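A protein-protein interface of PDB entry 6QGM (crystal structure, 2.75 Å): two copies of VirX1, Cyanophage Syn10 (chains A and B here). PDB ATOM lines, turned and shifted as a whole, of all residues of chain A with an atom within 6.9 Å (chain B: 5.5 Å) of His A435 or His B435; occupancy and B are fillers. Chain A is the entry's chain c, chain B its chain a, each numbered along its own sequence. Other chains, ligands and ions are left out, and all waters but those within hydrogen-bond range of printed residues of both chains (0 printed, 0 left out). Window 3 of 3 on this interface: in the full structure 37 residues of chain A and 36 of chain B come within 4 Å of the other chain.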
ATOM      1  N   GLU A 430     -13.146  -8.090 -24.590  1.00  0.00           N
ATOM      2  CA  GLU A 430     -11.765  -8.433 -24.140  1.00  0.00           C
ATOM      3  C   GLU A 430     -10.959  -7.141 -23.851  1.00  0.00           C
ATOM      4  O   GLU A 430      -9.908  -7.230 -23.193  1.00  0.00           O
ATOM      5  CB  GLU A 430     -11.079  -9.260 -25.227  1.00  0.00           C
ATOM      6  CG  GLU A 430     -11.762 -10.598 -25.500  1.00  0.00           C
ATOM      7  CD  GLU A 430     -10.993 -11.821 -25.038  1.00  0.00           C
ATOM      8  OE1 GLU A 430     -10.004 -11.666 -24.283  1.00  0.00           O
ATOM      9  OE2 GLU A 430     -11.365 -12.951 -25.467  1.00  0.00           O
ATOM     10  N   SER A 431     -11.446  -5.979 -24.302  1.00  0.00           N
ATOM     11  CA  SER A 431     -10.638  -4.742 -24.468  1.00  0.00           C
ATOM     12  C   SER A 431     -10.234  -4.137 -23.114  1.00  0.00           C
ATOM     13  O   SER A 431      -9.205  -3.431 -23.082  1.00  0.00           O
ATOM     14  CB  SER A 431     -11.358  -3.750 -25.331  1.00  0.00           C
ATOM     15  OG  SER A 431     -12.337  -3.033 -24.600  1.00  0.00           O
ATOM     16  N   MET A 432     -10.997  -4.384 -22.041  1.00  0.00           N
ATOM     17  CA  MET A 432     -10.708  -3.812 -20.696  1.00  0.00           C
ATOM     18  C   MET A 432      -9.673  -4.675 -19.952  1.00  0.00           C
ATOM     19  O   MET A 432      -9.215  -4.229 -18.889  1.00  0.00           O
ATOM     20  CB  MET A 432     -11.970  -3.705 -19.840  1.00  0.00           C
ATOM     21  CG  MET A 432     -12.927  -2.616 -20.291  1.00  0.00           C
ATOM     22  SD  MET A 432     -12.188  -0.970 -20.642  1.00  0.00           S
ATOM     23  CE  MET A 432     -12.439  -1.005 -22.409  1.00  0.00           C
ATOM     24  N   GLY A 433      -9.319  -5.847 -20.483  1.00  0.00           N
ATOM     25  CA  GLY A 433      -8.335  -6.752 -19.864  1.00  0.00           C
ATOM     26  C   GLY A 433      -6.907  -6.221 -19.971  1.00  0.00           C
ATOM     27  O   GLY A 433      -6.651  -5.254 -20.685  1.00  0.00           O
ATOM     28  N   PRO A 434      -5.929  -6.868 -19.298  1.00  0.00           N
ATOM     29  CA  PRO A 434      -4.542  -6.401 -19.303  1.00  0.00           C
ATOM     30  C   PRO A 434      -3.696  -6.806 -20.532  1.00  0.00           C
ATOM     31  O   PRO A 434      -2.630  -6.228 -20.708  1.00  0.00           O
ATOM     32  CB  PRO A 434      -3.994  -7.111 -18.063  1.00  0.00           C
ATOM     33  CG  PRO A 434      -4.691  -8.456 -18.094  1.00  0.00           C
ATOM     34  CD  PRO A 434      -6.101  -8.118 -18.536  1.00  0.00           C
ATOM     35  N   HIS A 435      -4.159  -7.790 -21.324  1.00  0.00           N
ATOM     36  CA  HIS A 435      -3.422  -8.414 -22.451  1.00  0.00           C
ATOM     37  C   HIS A 435      -3.859  -7.791 -23.779  1.00  0.00           C
ATOM     38  O   HIS A 435      -5.053  -7.509 -23.931  1.00  0.00           O
ATOM     39  CB  HIS A 435      -3.680  -9.923 -22.530  1.00  0.00           C
ATOM     40  CG  HIS A 435      -3.378 -10.677 -21.283  1.00  0.00           C
ATOM     41  ND1 HIS A 435      -2.266 -10.424 -20.509  1.00  0.00           N
ATOM     42  CD2 HIS A 435      -4.032 -11.686 -20.671  1.00  0.00           C
ATOM     43  CE1 HIS A 435      -2.265 -11.228 -19.461  1.00  0.00           C
ATOM     44  NE2 HIS A 435      -3.326 -12.014 -19.548  1.00  0.00           N
ATOM     45  N   ARG A 436      -2.922  -7.670 -24.727  1.00  0.00           N
ATOM     46  CA  ARG A 436      -3.193  -7.274 -26.133  1.00  0.00           C
ATOM     47  C   ARG A 436      -3.833  -8.449 -26.872  1.00  0.00           C
ATOM     48  O   ARG A 436      -3.320  -9.576 -26.757  1.00  0.00           O
ATOM     49  CB  ARG A 436      -1.912  -6.880 -26.864  1.00  0.00           C
ATOM     50  CG  ARG A 436      -1.426  -5.486 -26.508  1.00  0.00           C
ATOM     51  CD  ARG A 436      -0.531  -4.819 -27.536  1.00  0.00           C
ATOM     52  NE  ARG A 436       0.505  -4.051 -26.836  1.00  0.00           N
ATOM     53  CZ  ARG A 436       1.196  -3.047 -27.349  1.00  0.00           C
ATOM     54  NH1 ARG A 436       0.987  -2.648 -28.595  1.00  0.00           N
ATOM     55  NH2 ARG A 436       2.105  -2.446 -26.605  1.00  0.00           N
ATOM     56  N   GLN A 437      -4.878  -8.165 -27.644  1.00  0.00           N
ATOM     57  CA  GLN A 437      -5.674  -9.150 -28.413  1.00  0.00           C
ATOM     58  C   GLN A 437      -5.009  -9.361 -29.779  1.00  0.00           C
ATOM     59  O   GLN A 437      -4.512  -8.357 -30.349  1.00  0.00           O
ATOM     60  CB  GLN A 437      -7.094  -8.615 -28.611  1.00  0.00           C
ATOM     61  CG  GLN A 437      -8.074  -9.073 -27.557  1.00  0.00           C
ATOM     62  CD  GLN A 437      -7.496  -8.990 -26.169  1.00  0.00           C
ATOM     63  OE1 GLN A 437      -7.061  -9.997 -25.607  1.00  0.00           O
ATOM     64  NE2 GLN A 437      -7.470  -7.788 -25.613  1.00  0.00           N
ATOM     65  N   LYS A 438      -5.044 -10.589 -30.313  1.00  0.00           N
ATOM     66  CA  LYS A 438      -4.721 -10.850 -31.738  1.00  0.00           C
ATOM     67  C   LYS A 438      -5.625  -9.976 -32.622  1.00  0.00           C
ATOM     68  O   LYS A 438      -5.108  -9.326 -33.541  1.00  0.00           O
ATOM     69  CB  LYS A 438      -4.889 -12.327 -32.094  1.00  0.00           C
ATOM     70  CG  LYS A 438      -3.742 -13.198 -31.628  1.00  0.00           C
ATOM     71  CD  LYS A 438      -3.788 -14.626 -32.131  1.00  0.00           C
ATOM     72  CE  LYS A 438      -3.106 -15.599 -31.176  1.00  0.00           C
ATOM     73  NZ  LYS A 438      -1.618 -15.619 -31.262  1.00  0.00           N
ATOM     74  N   GLN A 439      -6.929 -10.004 -32.360  1.00  0.00           N
ATOM     75  CA  GLN A 439      -7.952  -9.252 -33.121  1.00  0.00           C
ATOM     76  C   GLN A 439      -8.297  -7.997 -32.326  1.00  0.00           C
ATOM     77  O   GLN A 439      -9.100  -8.090 -31.398  1.00  0.00           O
ATOM     78  CB  GLN A 439      -9.192 -10.107 -33.399  1.00  0.00           C
ATOM     79  CG  GLN A 439      -8.883 -11.456 -34.008  1.00  0.00           C
ATOM     80  CD  GLN A 439      -8.266 -11.336 -35.387  1.00  0.00           C
ATOM     81  OE1 GLN A 439      -8.522 -10.396 -36.154  1.00  0.00           O
ATOM     82  NE2 GLN A 439      -7.428 -12.308 -35.713  1.00  0.00           N
ATOM     83  N   GLN A 443     -10.540  -2.022 -30.856  1.00  0.00           N
ATOM     84  CA  GLN A 443      -9.711  -1.272 -29.880  1.00  0.00           C
ATOM     85  C   GLN A 443      -8.944  -0.177 -30.632  1.00  0.00           C
ATOM     86  O   GLN A 443      -8.902   0.971 -30.133  1.00  0.00           O
ATOM     87  CB  GLN A 443      -8.734  -2.204 -29.160  1.00  0.00           C
ATOM     88  CG  GLN A 443      -9.392  -3.243 -28.277  1.00  0.00           C
ATOM     89  CD  GLN A 443      -8.402  -4.240 -27.726  1.00  0.00           C
ATOM     90  OE1 GLN A 443      -8.781  -5.311 -27.271  1.00  0.00           O
ATOM     91  NE2 GLN A 443      -7.117  -3.916 -27.762  1.00  0.00           N
ATOM     92  N   GLU B 430       0.144 -21.816 -28.128  1.00  0.00           N
ATOM     93  CA  GLU B 430      -0.595 -20.628 -27.622  1.00  0.00           C
ATOM     94  C   GLU B 430      -1.246 -19.857 -28.777  1.00  0.00           C
ATOM     95  O   GLU B 430      -2.136 -19.020 -28.488  1.00  0.00           O
ATOM     96  CB  GLU B 430       0.319 -19.746 -26.764  1.00  0.00           C
ATOM     97  CG  GLU B 430       0.804 -20.436 -25.490  1.00  0.00           C
ATOM     98  CD  GLU B 430       0.009 -20.169 -24.214  1.00  0.00           C
ATOM     99  OE1 GLU B 430      -0.974 -19.378 -24.269  1.00  0.00           O
ATOM    100  OE2 GLU B 430       0.380 -20.743 -23.162  1.00  0.00           O
ATOM    101  N   GLY B 433      -5.080 -19.049 -29.431  1.00  0.00           N
ATOM    102  CA  GLY B 433      -5.762 -18.259 -28.387  1.00  0.00           C
ATOM    103  C   GLY B 433      -6.046 -16.834 -28.857  1.00  0.00           C
ATOM    104  O   GLY B 433      -5.607 -16.411 -29.928  1.00  0.00           O
ATOM    105  N   PRO B 434      -6.770 -16.025 -28.047  1.00  0.00           N
ATOM    106  CA  PRO B 434      -7.150 -14.670 -28.451  1.00  0.00           C
ATOM    107  C   PRO B 434      -6.085 -13.575 -28.237  1.00  0.00           C
ATOM    108  O   PRO B 434      -6.238 -12.507 -28.834  1.00  0.00           O
ATOM    109  CB  PRO B 434      -8.350 -14.419 -27.535  1.00  0.00           C
ATOM    110  CG  PRO B 434      -7.953 -15.096 -26.274  1.00  0.00           C
ATOM    111  CD  PRO B 434      -7.230 -16.361 -26.693  1.00  0.00           C
ATOM    112  N   HIS B 435      -5.056 -13.850 -27.424  1.00  0.00           N
ATOM    113  CA  HIS B 435      -4.040 -12.881 -26.932  1.00  0.00           C
ATOM    114  C   HIS B 435      -2.761 -12.960 -27.763  1.00  0.00           C
ATOM    115  O   HIS B 435      -2.398 -14.086 -28.154  1.00  0.00           O
ATOM    116  CB  HIS B 435      -3.647 -13.179 -25.473  1.00  0.00           C
ATOM    117  CG  HIS B 435      -4.785 -13.202 -24.515  1.00  0.00           C
ATOM    118  ND1 HIS B 435      -5.804 -12.269 -24.564  1.00  0.00           N
ATOM    119  CD2 HIS B 435      -5.053 -14.028 -23.482  1.00  0.00           C
ATOM    120  CE1 HIS B 435      -6.663 -12.522 -23.601  1.00  0.00           C
ATOM    121  NE2 HIS B 435      -6.219 -13.595 -22.916  1.00  0.00           N
ATOM    122  N   ARG B 436      -2.059 -11.833 -27.920  1.00  0.00           N
ATOM    123  CA  ARG B 436      -0.707 -11.764 -28.526  1.00  0.00           C
ATOM    124  C   ARG B 436       0.339 -12.315 -27.553  1.00  0.00           C
ATOM    125  O   ARG B 436       0.321 -11.902 -26.393  1.00  0.00           O
ATOM    126  CB  ARG B 436      -0.345 -10.326 -28.901  1.00  0.00           C
ATOM    127  CG  ARG B 436      -0.905  -9.938 -30.255  1.00  0.00           C
ATOM    128  CD  ARG B 436      -0.813  -8.457 -30.549  1.00  0.00           C
ATOM    129  NE  ARG B 436      -2.009  -7.981 -31.258  1.00  0.00           N
ATOM    130  CZ  ARG B 436      -2.027  -7.135 -32.283  1.00  0.00           C
ATOM    131  NH1 ARG B 436      -0.892  -6.658 -32.758  1.00  0.00           N
ATOM    132  NH2 ARG B 436      -3.188  -6.805 -32.823  1.00  0.00           N
ATOM    133  N   GLN B 437       1.234 -13.162 -28.070  1.00  0.00           N
ATOM    134  CA  GLN B 437       2.318 -13.817 -27.303  1.00  0.00           C
ATOM    135  C   GLN B 437       3.543 -12.909 -27.295  1.00  0.00           C
ATOM    136  O   GLN B 437       3.815 -12.284 -28.338  1.00  0.00           O
ATOM    137  CB  GLN B 437       2.680 -15.160 -27.946  1.00  0.00           C
ATOM    138  CG  GLN B 437       1.948 -16.342 -27.335  1.00  0.00           C
ATOM    139  CD  GLN B 437       0.488 -16.043 -27.083  1.00  0.00           C
ATOM    140  OE1 GLN B 437       0.049 -15.741 -25.976  1.00  0.00           O
ATOM    141  NE2 GLN B 437      -0.282 -16.116 -28.144  1.00  0.00           N
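O of Pro B434 sits at hydrogen-bond distance from N of Lys A438 (2.7 Å).
The side-chain amide oxygen (OE1) of Gln A437 is in hydrogen-bond range of a ring nitrogen (ND1) of His B435, at 2.8 Å.
The backbone carbonyl oxygen of Arg A436 is in hydrogen-bond range of the backbone NH of Arg B436, 2.8 Å away.
The backbone carbonyl oxygen of Gln A437 sits at hydrogen-bond distance from the guanidinium group of Arg B436.
NH2 of Arg B436 is in hydrogen-bond range of O of Lys A438 (3.2 Å).
The side-chain amino group (NZ) of Lys A438 lies close to the side-chain amide nitrogen (NE2) of Gln B437.
NE2 of Gln B437 sits at hydrogen-bond distance from O of Glu B430.
The backbone carbonyl oxygen of His B435 sits at hydrogen-bond distance from the side-chain amide nitrogen of Gln B437.
NE2 of Gln A437 sits at hydrogen-bond distance from O of Glu A430, 3.5 Å away.
The backbone carbonyl oxygen (O) of His A435 is in hydrogen-bond range of the side-chain amide nitrogen (NE2) of Gln A437, 3.0 Å away.
The side-chain amide nitrogen (NE2) of Gln A437 sits at hydrogen-bond distance from the side-chain amide oxygen (OE1) of Gln A443, 3.3 Å away.
Among the printed residues, pairs that only touch across the chains: Lys A438 with Gly B433 (2.9 Å), Arg A436 with His B435 (3.4 Å), Gln A437 with Pro B434 (3.4 Å), Lys A438 with His B435 (3.5 Å), Glu A430 with His B435 (3.5 Å), His A435 with His B435 (3.7 Å) and Glu A430 with Pro B434 (3.9 Å).
Printed residues of chain B within 4 Å of His A435: His B435 (3.7 Å).
His B435 touches just these residues of chain A: Glu A430 (3.5 Å), His A435 (3.7 Å), Arg A436 (3.4 Å), Gln A437 (2.8 Å) and Lys A438 (3.5 Å).
Of the printed residues of chain A, Pro B434 touches Glu A430 (3.9 Å), Gln A437 (3.4 Å) and Lys A438 (2.7 Å).
Of the printed residues of chain B, Glu A430 touches Pro B434 and His B435.
Of the printed residues of chain B, Gln A437 touches Pro B434, His B435 and Arg B436.
Of the printed residues of chain B, Lys A438 touches Gly B433 (2.9 Å), Pro B434 (2.7 Å), His B435 (3.5 Å), Arg B436 (3.2 Å) and Gln B437 (3.4 Å).
Met A432 touches none of the printed residues of chain B.
Ser A431 touches none of the printed residues of chain B.
The nearest residue of chain A that does not touch His B435 is Gln A439 (6.5 Å).
The nearest printed residue of chain A that does not touch Pro B434 is Gln A439 (4.4 Å).
Hydrophobic or aromatic side chains of chain B within 4 Å of the printed part of chain A: Pro B434 and His B435.
Of the 11 printed residues of chain A, 5 touch a printed residue of chain B.
Printed residues of chain A that touch a printed residue of chain B: Glu A430, His A435, Arg A436, Gln A437 and Lys A438.
Hydrophobic or aromatic side chains of chain A within 4 Å of the printed part of chain B: His A435.
Glu A430 touches His B435, but with the chains exchanged His A435 does not touch Glu B430 (9.0 Å).
His A435 touches its own counterpart, His B435.
Arg A436 touches His B435, but with the chains exchanged His A435 does not touch Arg B436 (5.9 Å).
Gln A437 touches Arg B436, but with the chains exchanged Arg A436 does not touch Gln B437 (5.9 Å).
Positions printed for both chains: 430, 433, 434, 435, 436 and 437.
Of the 13 pairs that touch across the chains among the printed residues, 2 have their exchanged pair printed and touching as well.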
